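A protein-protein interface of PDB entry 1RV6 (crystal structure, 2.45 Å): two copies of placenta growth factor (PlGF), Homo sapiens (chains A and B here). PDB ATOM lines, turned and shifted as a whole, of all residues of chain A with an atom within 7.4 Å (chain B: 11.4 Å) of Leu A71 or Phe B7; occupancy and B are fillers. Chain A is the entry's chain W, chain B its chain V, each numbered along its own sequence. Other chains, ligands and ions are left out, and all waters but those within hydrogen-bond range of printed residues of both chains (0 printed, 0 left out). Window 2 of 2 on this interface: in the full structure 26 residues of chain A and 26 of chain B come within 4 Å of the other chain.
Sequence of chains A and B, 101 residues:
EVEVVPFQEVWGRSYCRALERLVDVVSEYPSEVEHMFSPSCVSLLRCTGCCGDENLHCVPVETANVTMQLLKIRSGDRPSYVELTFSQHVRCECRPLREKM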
ATOM      1  N   MET A  36      20.060 -15.690  -4.890  1.00  0.00           N
ATOM      2  CA  MET A  36      20.535 -15.701  -6.273  1.00  0.00           C
ATOM      3  C   MET A  36      19.447 -16.195  -7.215  1.00  0.00           C
ATOM      4  O   MET A  36      18.662 -17.065  -6.850  1.00  0.00           O
ATOM      5  CB  MET A  36      21.749 -16.599  -6.443  1.00  0.00           C
ATOM      6  CG  MET A  36      23.007 -16.134  -5.756  1.00  0.00           C
ATOM      7  SD  MET A  36      24.367 -17.168  -6.275  1.00  0.00           S
ATOM      8  CE  MET A  36      24.114 -18.586  -5.183  1.00  0.00           C
ATOM      9  N   PHE A  37      19.410 -15.638  -8.424  1.00  0.00           N
ATOM     10  CA  PHE A  37      18.430 -16.020  -9.420  1.00  0.00           C
ATOM     11  C   PHE A  37      19.163 -16.536 -10.601  1.00  0.00           C
ATOM     12  O   PHE A  37      20.294 -16.111 -10.894  1.00  0.00           O
ATOM     13  CB  PHE A  37      17.544 -14.836  -9.832  1.00  0.00           C
ATOM     14  CG  PHE A  37      16.628 -14.398  -8.740  1.00  0.00           C
ATOM     15  CD1 PHE A  37      15.354 -14.965  -8.621  1.00  0.00           C
ATOM     16  CD2 PHE A  37      17.073 -13.510  -7.766  1.00  0.00           C
ATOM     17  CE1 PHE A  37      14.523 -14.621  -7.571  1.00  0.00           C
ATOM     18  CE2 PHE A  37      16.239 -13.150  -6.707  1.00  0.00           C
ATOM     19  CZ  PHE A  37      14.953 -13.697  -6.620  1.00  0.00           C
ATOM     20  N   SER A  38      18.509 -17.458 -11.288  1.00  0.00           N
ATOM     21  CA  SER A  38      19.092 -18.019 -12.477  1.00  0.00           C
ATOM     22  C   SER A  38      18.064 -17.960 -13.618  1.00  0.00           C
ATOM     23  O   SER A  38      17.010 -18.589 -13.515  1.00  0.00           O
ATOM     24  CB  SER A  38      19.559 -19.434 -12.182  1.00  0.00           C
ATOM     25  OG  SER A  38      19.929 -20.065 -13.375  1.00  0.00           O
ATOM     26  N   PRO A  39      18.353 -17.199 -14.683  1.00  0.00           N
ATOM     27  CA  PRO A  39      19.633 -16.482 -14.850  1.00  0.00           C
ATOM     28  C   PRO A  39      19.635 -15.226 -13.960  1.00  0.00           C
ATOM     29  O   PRO A  39      18.575 -14.899 -13.431  1.00  0.00           O
ATOM     30  CB  PRO A  39      19.615 -16.076 -16.334  1.00  0.00           C
ATOM     31  CG  PRO A  39      18.134 -15.920 -16.695  1.00  0.00           C
ATOM     32  CD  PRO A  39      17.410 -16.936 -15.792  1.00  0.00           C
ATOM     33  N   SER A  40      20.771 -14.550 -13.786  1.00  0.00           N
ATOM     34  CA  SER A  40      20.839 -13.406 -12.863  1.00  0.00           C
ATOM     35  C   SER A  40      20.446 -12.151 -13.591  1.00  0.00           C
ATOM     36  O   SER A  40      20.194 -11.091 -12.989  1.00  0.00           O
ATOM     37  CB  SER A  40      22.233 -13.245 -12.231  1.00  0.00           C
ATOM     38  OG  SER A  40      23.277 -13.272 -13.198  1.00  0.00           O
ATOM     39  N   MET A  68       8.058 -13.631 -15.993  1.00  0.00           N
ATOM     40  CA  MET A  68       9.149 -14.504 -16.412  1.00  0.00           C
ATOM     41  C   MET A  68       9.352 -15.629 -15.432  1.00  0.00           C
ATOM     42  O   MET A  68       9.237 -15.436 -14.213  1.00  0.00           O
ATOM     43  CB  MET A  68      10.430 -13.696 -16.524  1.00  0.00           C
ATOM     44  CG  MET A  68      10.338 -12.671 -17.606  1.00  0.00           C
ATOM     45  SD  MET A  68      11.934 -12.182 -18.066  1.00  0.00           S
ATOM     46  CE  MET A  68      11.489 -10.611 -18.998  1.00  0.00           C
ATOM     47  N   GLN A  69       9.638 -16.802 -15.986  1.00  0.00           N
ATOM     48  CA  GLN A  69       9.922 -17.996 -15.212  1.00  0.00           C
ATOM     49  C   GLN A  69      11.396 -17.972 -14.874  1.00  0.00           C
ATOM     50  O   GLN A  69      12.227 -17.882 -15.783  1.00  0.00           O
ATOM     51  CB  GLN A  69       9.618 -19.253 -16.060  1.00  0.00           C
ATOM     52  CG  GLN A  69       8.141 -19.589 -16.200  1.00  0.00           C
ATOM     53  CD  GLN A  69       7.860 -20.849 -17.028  1.00  0.00           C
ATOM     54  OE1 GLN A  69       8.768 -21.627 -17.340  1.00  0.00           O
ATOM     55  NE2 GLN A  69       6.594 -21.048 -17.378  1.00  0.00           N
ATOM     56  N   LEU A  70      11.720 -18.079 -13.587  1.00  0.00           N
ATOM     57  CA  LEU A  70      13.109 -18.138 -13.114  1.00  0.00           C
ATOM     58  C   LEU A  70      13.326 -19.226 -12.050  1.00  0.00           C
ATOM     59  O   LEU A  70      12.379 -19.820 -11.520  1.00  0.00           O
ATOM     60  CB  LEU A  70      13.540 -16.807 -12.465  1.00  0.00           C
ATOM     61  CG  LEU A  70      13.663 -15.409 -13.084  1.00  0.00           C
ATOM     62  CD1 LEU A  70      14.854 -15.291 -13.960  1.00  0.00           C
ATOM     63  CD2 LEU A  70      12.410 -15.022 -13.823  1.00  0.00           C
ATOM     64  N   LEU A  71      14.597 -19.421 -11.711  1.00  0.00           N
ATOM     65  CA  LEU A  71      15.037 -20.269 -10.621  1.00  0.00           C
ATOM     66  C   LEU A  71      15.631 -19.390  -9.536  1.00  0.00           C
ATOM     67  O   LEU A  71      16.438 -18.482  -9.823  1.00  0.00           O
ATOM     68  CB  LEU A  71      16.097 -21.263 -11.139  1.00  0.00           C
ATOM     69  CG  LEU A  71      15.759 -22.756 -11.326  1.00  0.00           C
ATOM     70  CD1 LEU A  71      14.270 -23.111 -11.209  1.00  0.00           C
ATOM     71  CD2 LEU A  71      16.325 -23.264 -12.608  1.00  0.00           C
ATOM     72  N   LYS A  72      15.229 -19.646  -8.295  1.00  0.00           N
ATOM     73  CA  LYS A  72      15.759 -18.920  -7.134  1.00  0.00           C
ATOM     74  C   LYS A  72      16.616 -19.850  -6.268  1.00  0.00           C
ATOM     75  O   LYS A  72      16.147 -20.889  -5.812  1.00  0.00           O
ATOM     76  CB  LYS A  72      14.634 -18.334  -6.290  1.00  0.00           C
ATOM     77  CG  LYS A  72      15.133 -17.430  -5.145  1.00  0.00           C
ATOM     78  CD  LYS A  72      13.974 -16.762  -4.406  1.00  0.00           C
ATOM     79  CE  LYS A  72      14.492 -15.670  -3.521  1.00  0.00           C
ATOM     80  NZ  LYS A  72      13.479 -15.189  -2.530  1.00  0.00           N
ATOM     81  N   ILE A  73      17.865 -19.476  -6.054  1.00  0.00           N
ATOM     82  CA  ILE A  73      18.791 -20.290  -5.264  1.00  0.00           C
ATOM     83  C   ILE A  73      18.981 -19.580  -3.920  1.00  0.00           C
ATOM     84  O   ILE A  73      19.168 -18.365  -3.865  1.00  0.00           O
ATOM     85  CB  ILE A  73      20.118 -20.532  -6.052  1.00  0.00           C
ATOM     86  CG1 ILE A  73      19.807 -21.109  -7.442  1.00  0.00           C
ATOM     87  CG2 ILE A  73      21.132 -21.443  -5.294  1.00  0.00           C
ATOM     88  CD1 ILE A  73      20.986 -20.979  -8.428  1.00  0.00           C
ATOM     89  N   PRO A  79      16.076 -24.772  -3.408  1.00  0.00           N
ATOM     90  CA  PRO A  79      15.829 -23.820  -4.495  1.00  0.00           C
ATOM     91  C   PRO A  79      14.345 -23.832  -4.938  1.00  0.00           C
ATOM     92  O   PRO A  79      13.644 -24.771  -4.590  1.00  0.00           O
ATOM     93  CB  PRO A  79      16.745 -24.325  -5.624  1.00  0.00           C
ATOM     94  CG  PRO A  79      16.955 -25.818  -5.342  1.00  0.00           C
ATOM     95  CD  PRO A  79      16.834 -25.970  -3.843  1.00  0.00           C
ATOM     96  N   SER A  80      13.880 -22.830  -5.690  1.00  0.00           N
ATOM     97  CA  SER A  80      12.473 -22.803  -6.158  1.00  0.00           C
ATOM     98  C   SER A  80      12.295 -22.255  -7.561  1.00  0.00           C
ATOM     99  O   SER A  80      12.986 -21.313  -7.993  1.00  0.00           O
ATOM    100  CB  SER A  80      11.590 -21.929  -5.261  1.00  0.00           C
ATOM    101  OG  SER A  80      11.575 -22.377  -3.927  1.00  0.00           O
ATOM    102  N   TYR A  81      11.322 -22.849  -8.250  1.00  0.00           N
ATOM    103  CA  TYR A  81      10.712 -22.266  -9.432  1.00  0.00           C
ATOM    104  C   TYR A  81       9.950 -21.046  -8.967  1.00  0.00           C
ATOM    105  O   TYR A  81       9.217 -21.095  -7.983  1.00  0.00           O
ATOM    106  CB  TYR A  81       9.768 -23.268 -10.077  1.00  0.00           C
ATOM    107  CG  TYR A  81       8.907 -22.730 -11.196  1.00  0.00           C
ATOM    108  CD1 TYR A  81       9.355 -22.756 -12.516  1.00  0.00           C
ATOM    109  CD2 TYR A  81       7.622 -22.207 -10.935  1.00  0.00           C
ATOM    110  CE1 TYR A  81       8.548 -22.270 -13.562  1.00  0.00           C
ATOM    111  CE2 TYR A  81       6.819 -21.709 -11.957  1.00  0.00           C
ATOM    112  CZ  TYR A  81       7.286 -21.751 -13.271  1.00  0.00           C
ATOM    113  OH  TYR A  81       6.500 -21.278 -14.296  1.00  0.00           O
ATOM    114  N   VAL A  82      10.130 -19.949  -9.685  1.00  0.00           N
ATOM    115  CA  VAL A  82       9.564 -18.670  -9.284  1.00  0.00           C
ATOM    116  C   VAL A  82       9.032 -17.954 -10.560  1.00  0.00           C
ATOM    117  O   VAL A  82       9.515 -18.194 -11.676  1.00  0.00           O
ATOM    118  CB  VAL A  82      10.707 -17.904  -8.554  1.00  0.00           C
ATOM    119  CG1 VAL A  82      11.290 -16.766  -9.375  1.00  0.00           C
ATOM    120  CG2 VAL A  82      10.341 -17.528  -7.163  1.00  0.00           C
ATOM    121  N   GLU A  83       8.032 -17.105 -10.418  1.00  0.00           N
ATOM    122  CA  GLU A  83       7.545 -16.305 -11.548  1.00  0.00           C
ATOM    123  C   GLU A  83       7.578 -14.843 -11.095  1.00  0.00           C
ATOM    124  O   GLU A  83       6.899 -14.486 -10.132  1.00  0.00           O
ATOM    125  CB  GLU A  83       6.120 -16.709 -11.970  1.00  0.00           C
ATOM    126  CG  GLU A  83       6.033 -17.969 -12.833  1.00  0.00           C
ATOM    127  CD  GLU A  83       4.617 -18.342 -13.247  1.00  0.00           C
ATOM    128  OE1 GLU A  83       3.735 -17.460 -13.258  1.00  0.00           O
ATOM    129  OE2 GLU A  83       4.364 -19.534 -13.553  1.00  0.00           O
ATOM    130  N   VAL B   4       3.245 -15.752 -19.829  1.00  0.00           N
ATOM    131  CA  VAL B   4       4.496 -16.104 -19.093  1.00  0.00           C
ATOM    132  C   VAL B   4       5.606 -16.631 -20.018  1.00  0.00           C
ATOM    133  O   VAL B   4       5.420 -17.618 -20.744  1.00  0.00           O
ATOM    134  CB  VAL B   4       4.220 -17.121 -17.976  1.00  0.00           C
ATOM    135  CG1 VAL B   4       5.438 -17.248 -17.033  1.00  0.00           C
ATOM    136  CG2 VAL B   4       2.976 -16.729 -17.207  1.00  0.00           C
ATOM    137  N   VAL B   5       6.758 -15.967 -19.987  1.00  0.00           N
ATOM    138  CA  VAL B   5       7.916 -16.414 -20.763  1.00  0.00           C
ATOM    139  C   VAL B   5       8.460 -17.678 -20.113  1.00  0.00           C
ATOM    140  O   VAL B   5       8.816 -17.645 -18.945  1.00  0.00           O
ATOM    141  CB  VAL B   5       9.025 -15.332 -20.858  1.00  0.00           C
ATOM    142  CG1 VAL B   5      10.124 -15.766 -21.831  1.00  0.00           C
ATOM    143  CG2 VAL B   5       8.444 -13.987 -21.275  1.00  0.00           C
ATOM    144  N   PRO B   6       8.485 -18.805 -20.838  1.00  0.00           N
ATOM    145  CA  PRO B   6       8.967 -20.069 -20.254  1.00  0.00           C
ATOM    146  C   PRO B   6      10.468 -19.990 -19.985  1.00  0.00           C
ATOM    147  O   PRO B   6      11.194 -19.279 -20.710  1.00  0.00           O
ATOM    148  CB  PRO B   6       8.643 -21.114 -21.325  1.00  0.00           C
ATOM    149  CG  PRO B   6       8.578 -20.364 -22.568  1.00  0.00           C
ATOM    150  CD  PRO B   6       8.066 -18.980 -22.241  1.00  0.00           C
ATOM    151  N   PHE B   7      10.911 -20.698 -18.949  1.00  0.00           N
ATOM    152  CA  PHE B   7      12.271 -20.593 -18.452  1.00  0.00           C
ATOM    153  C   PHE B   7      13.347 -20.679 -19.518  1.00  0.00           C
ATOM    154  O   PHE B   7      14.326 -19.939 -19.477  1.00  0.00           O
ATOM    155  CB  PHE B   7      12.543 -21.671 -17.419  1.00  0.00           C
ATOM    156  CG  PHE B   7      13.970 -21.675 -16.932  1.00  0.00           C
ATOM    157  CD1 PHE B   7      14.374 -20.799 -15.937  1.00  0.00           C
ATOM    158  CD2 PHE B   7      14.910 -22.549 -17.477  1.00  0.00           C
ATOM    159  CE1 PHE B   7      15.688 -20.795 -15.487  1.00  0.00           C
ATOM    160  CE2 PHE B   7      16.239 -22.532 -17.044  1.00  0.00           C
ATOM    161  CZ  PHE B   7      16.620 -21.656 -16.032  1.00  0.00           C
ATOM    162  N   GLN B   8      13.178 -21.593 -20.466  1.00  0.00           N
ATOM    163  CA  GLN B   8      14.196 -21.783 -21.467  1.00  0.00           C
ATOM    164  C   GLN B   8      14.302 -20.598 -22.397  1.00  0.00           C
ATOM    165  O   GLN B   8      15.385 -20.307 -22.937  1.00  0.00           O
ATOM    166  CB  GLN B   8      14.014 -23.110 -22.196  1.00  0.00           C
ATOM    167  CG  GLN B   8      14.503 -24.270 -21.326  1.00  0.00           C
ATOM    168  CD  GLN B   8      14.255 -25.637 -21.925  1.00  0.00           C
ATOM    169  OE1 GLN B   8      14.628 -25.901 -23.075  1.00  0.00           O
ATOM    170  NE2 GLN B   8      13.652 -26.525 -21.133  1.00  0.00           N
ATOM    171  N   GLU B   9      13.201 -19.879 -22.562  1.00  0.00           N
ATOM    172  CA  GLU B   9      13.262 -18.641 -23.337  1.00  0.00           C
ATOM    173  C   GLU B   9      13.928 -17.544 -22.513  1.00  0.00           C
ATOM    174  O   GLU B   9      14.695 -16.760 -23.050  1.00  0.00           O
ATOM    175  CB  GLU B   9      11.883 -18.210 -23.827  1.00  0.00           C
ATOM    176  CG  GLU B   9      11.331 -19.098 -24.940  1.00  0.00           C
ATOM    177  CD  GLU B   9      10.075 -18.536 -25.596  1.00  0.00           C
ATOM    178  OE1 GLU B   9       9.898 -17.291 -25.613  1.00  0.00           O
ATOM    179  OE2 GLU B   9       9.273 -19.347 -26.110  1.00  0.00           O
ATOM    180  N   VAL B  10      13.657 -17.520 -21.202  1.00  0.00           N
ATOM    181  CA  VAL B  10      14.216 -16.507 -20.323  1.00  0.00           C
ATOM    182  C   VAL B  10      15.709 -16.683 -20.395  1.00  0.00           C
ATOM    183  O   VAL B  10      16.455 -15.700 -20.552  1.00  0.00           O
ATOM    184  CB  VAL B  10      13.759 -16.626 -18.841  1.00  0.00           C
ATOM    185  CG1 VAL B  10      14.525 -15.622 -17.982  1.00  0.00           C
ATOM    186  CG2 VAL B  10      12.252 -16.417 -18.709  1.00  0.00           C
ATOM    187  N   TRP B  11      16.126 -17.945 -20.271  1.00  0.00           N
ATOM    188  CA  TRP B  11      17.533 -18.328 -20.340  1.00  0.00           C
ATOM    189  C   TRP B  11      18.168 -17.910 -21.665  1.00  0.00           C
ATOM    190  O   TRP B  11      19.164 -17.203 -21.661  1.00  0.00           O
ATOM    191  CB  TRP B  11      17.697 -19.837 -20.164  1.00  0.00           C
ATOM    192  CG  TRP B  11      19.157 -20.243 -20.097  1.00  0.00           C
ATOM    193  CD1 TRP B  11      19.921 -20.730 -21.116  1.00  0.00           C
ATOM    194  CD2 TRP B  11      20.023 -20.144 -18.959  1.00  0.00           C
ATOM    195  NE1 TRP B  11      21.209 -20.955 -20.684  1.00  0.00           N
ATOM    196  CE2 TRP B  11      21.300 -20.610 -19.360  1.00  0.00           C
ATOM    197  CE3 TRP B  11      19.850 -19.724 -17.633  1.00  0.00           C
ATOM    198  CZ2 TRP B  11      22.402 -20.665 -18.479  1.00  0.00           C
ATOM    199  CZ3 TRP B  11      20.949 -19.778 -16.744  1.00  0.00           C
ATOM    200  CH2 TRP B  11      22.202 -20.241 -17.180  1.00  0.00           C
ATOM    201  N   GLY B  12      17.592 -18.368 -22.786  1.00  0.00           N
ATOM    202  CA  GLY B  12      18.115 -18.077 -24.112  1.00  0.00           C
ATOM    203  C   GLY B  12      18.242 -16.583 -24.391  1.00  0.00           C
ATOM    204  O   GLY B  12      19.083 -16.144 -25.180  1.00  0.00           O
ATOM    205  N   ARG B  13      17.383 -15.798 -23.746  1.00  0.00           N
ATOM    206  CA  ARG B  13      17.289 -14.376 -24.014  1.00  0.00           C
ATOM    207  C   ARG B  13      18.403 -13.574 -23.324  1.00  0.00           C
ATOM    208  O   ARG B  13      18.690 -12.459 -23.747  1.00  0.00           O
ATOM    209  CB  ARG B  13      15.868 -13.861 -23.650  1.00  0.00           C
ATOM    210  CG  ARG B  13      14.895 -13.803 -24.870  1.00  0.00           C
ATOM    211  CD  ARG B  13      13.454 -14.331 -24.709  1.00  0.00           C
ATOM    212  NE  ARG B  13      12.486 -13.264 -24.511  1.00  0.00           N
ATOM    213  CZ  ARG B  13      11.162 -13.336 -24.729  1.00  0.00           C
ATOM    214  NH1 ARG B  13      10.554 -14.444 -25.175  1.00  0.00           N
ATOM    215  NH2 ARG B  13      10.433 -12.253 -24.500  1.00  0.00           N
ATOM    216  N   SER B  14      19.044 -14.141 -22.294  1.00  0.00           N
ATOM    217  CA  SER B  14      20.014 -13.387 -21.472  1.00  0.00           C
ATOM    218  C   SER B  14      21.388 -14.030 -21.386  1.00  0.00           C
ATOM    219  O   SER B  14      22.309 -13.422 -20.827  1.00  0.00           O
ATOM    220  CB  SER B  14      19.495 -13.216 -20.051  1.00  0.00           C
ATOM    221  OG  SER B  14      19.436 -14.475 -19.410  1.00  0.00           O
ATOM    222  N   TYR B  15      21.526 -15.236 -21.941  1.00  0.00           N
ATOM    223  CA  TYR B  15      22.710 -16.065 -21.729  1.00  0.00           C
ATOM    224  C   TYR B  15      23.989 -15.518 -22.382  1.00  0.00           C
ATOM    225  O   TYR B  15      24.926 -15.118 -21.679  1.00  0.00           O
ATOM    226  CB  TYR B  15      22.468 -17.482 -22.215  1.00  0.00           C
ATOM    227  CG  TYR B  15      23.699 -18.338 -22.104  1.00  0.00           C
ATOM    228  CD1 TYR B  15      24.239 -18.679 -20.840  1.00  0.00           C
ATOM    229  CD2 TYR B  15      24.342 -18.814 -23.260  1.00  0.00           C
ATOM    230  CE1 TYR B  15      25.396 -19.475 -20.741  1.00  0.00           C
ATOM    231  CE2 TYR B  15      25.493 -19.593 -23.171  1.00  0.00           C
ATOM    232  CZ  TYR B  15      26.015 -19.922 -21.913  1.00  0.00           C
ATOM    233  OH  TYR B  15      27.147 -20.689 -21.850  1.00  0.00           O
ATOM    234  N   ARG B  17      24.625 -13.635 -26.347  1.00  0.00           N
ATOM    235  CA  ARG B  17      24.162 -13.475 -27.722  1.00  0.00           C
ATOM    236  C   ARG B  17      24.516 -12.161 -28.361  1.00  0.00           C
ATOM    237  O   ARG B  17      24.819 -11.187 -27.660  1.00  0.00           O
ATOM    238  CB  ARG B  17      22.659 -13.664 -27.805  1.00  0.00           C
ATOM    239  CG  ARG B  17      21.865 -12.871 -26.821  1.00  0.00           C
ATOM    240  CD  ARG B  17      20.568 -12.480 -27.464  1.00  0.00           C
ATOM    241  NE  ARG B  17      19.527 -12.059 -26.555  1.00  0.00           N
ATOM    242  CZ  ARG B  17      18.365 -11.555 -26.942  1.00  0.00           C
ATOM    243  NH1 ARG B  17      18.096 -11.393 -28.243  1.00  0.00           N
ATOM    244  NH2 ARG B  17      17.466 -11.203 -26.019  1.00  0.00           N
ATOM    245  N   CYS B  50      24.621 -12.799 -19.366  1.00  0.00           N
ATOM    246  CA  CYS B  50      25.087 -13.170 -18.030  1.00  0.00           C
ATOM    247  C   CYS B  50      25.870 -14.484 -17.987  1.00  0.00           C
ATOM    248  O   CYS B  50      26.513 -14.781 -16.974  1.00  0.00           O
ATOM    249  CB  CYS B  50      23.977 -13.130 -16.973  1.00  0.00           C
ATOM    250  SG  CYS B  50      22.285 -13.187 -17.603  1.00  0.00           S
ATOM    251  N   CYS B  51      25.836 -15.255 -19.078  1.00  0.00           N
ATOM    252  CA  CYS B  51      26.741 -16.406 -19.249  1.00  0.00           C
ATOM    253  C   CYS B  51      26.612 -17.520 -18.208  1.00  0.00           C
ATOM    254  O   CYS B  51      27.458 -18.424 -18.124  1.00  0.00           O
ATOM    255  CB  CYS B  51      28.197 -15.922 -19.312  1.00  0.00           C
ATOM    256  SG  CYS B  51      28.755 -15.538 -20.988  1.00  0.00           S
ATOM    257  N   GLY B  52      25.551 -17.459 -17.410  1.00  0.00           N
ATOM    258  CA  GLY B  52      25.331 -18.429 -16.346  1.00  0.00           C
ATOM    259  C   GLY B  52      26.333 -18.376 -15.220  1.00  0.00           C
ATOM    260  O   GLY B  52      26.290 -19.208 -14.302  1.00  0.00           O
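N of Cys B50 is in hydrogen-bond range of O of Tyr B15 (3.3 Å). The side-chain amide nitrogen of Gln A69 sits close to the side-chain hydroxyl of Tyr A81 (3.1 Å). The backbone carbonyl oxygen of Ser B14 lies within hydrogen-bond range of the backbone NH of Cys B50, at 2.8 Å. O of Val B10 lies within hydrogen-bond range of OG of Ser B14, 3.4 Å away. The backbone carbonyl oxygen of Leu A71 sits at hydrogen-bond distance from the backbone NH of Ser A38 (2.7 Å).
The side-chain amide oxygen (OE1) of Gln A69 lies within hydrogen-bond range of the backbone NH (N) of Phe B7 (2.8 Å). O of Val B5 sits at hydrogen-bond distance from N of Gln A69, 3.2 Å away.
No position is printed for both chains.
Phe B7 touches Ser A38 (CE1 to O, 3.2 Å). Trp B11 touches Ser A38. Pro A39 touches Val B10 (CG to CG1, 3.8 Å). Trp B11 touches Pro A39. OG of Ser B14 touches CG of Pro A39, at 3.3 Å. Cys B50 touches Ser A40. Val B10 touches Met A68. CG of Gln A69 touches CG1 of Val B4 (3.7 Å). Gln A69 touches Pro B6 (OE1 to CA, 3.3 Å). Gln A69 touches Val B10.
Hydrophobic or aromatic side chains of chain A that line the printed part of chain B: Pro A39, Met A68 and Leu A71. Among the printed residues, 13 pairs touch across the chains. Among the printed residues, no Asp or Glu carboxylate lies within 4 Å of a Lys or Arg side-chain nitrogen of the other chain.
Of the printed residues of chain B, Leu A71 touches Phe B7. Phe B7 touches just these residues of chain A: Ser A38 (3.2 Å), Gln A69 (2.8 Å) and Leu A71 (3.8 Å). Phe A37 touches none of the printed residues of chain B. Ser A38 touches two residues of chain B. Of chain B, only Val B10, Trp B11 and Ser B14 come within 4 Å of Pro A39. Gln A69 touches just these residues of chain B: Val B4 (3.7 Å), Val B5 (3.2 Å), Pro B6 (3.3 Å), Phe B7 (2.8 Å) and Val B10 (3.3 Å). No residue of chain B comes within 4 Å of Ile A73. Val A82 touches none of the printed residues of chain B. Printed residues of chain A within 4 Å of Val B5: Gln A69 (3.2 Å). Printed residues of chain A within 4 Å of Trp B11: Ser A38 (3.5 Å) and Pro A39 (3.9 Å). Printed residues of chain A within 4 Å of Pro B6: Gln A69. Printed residues of chain A within 4 Å of Val B4: Gln A69. Printed residues of chain A within 4 Å of Cys B50: Ser A40 (3.8 Å). Arg B17 touches none of the printed residues of chain A.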
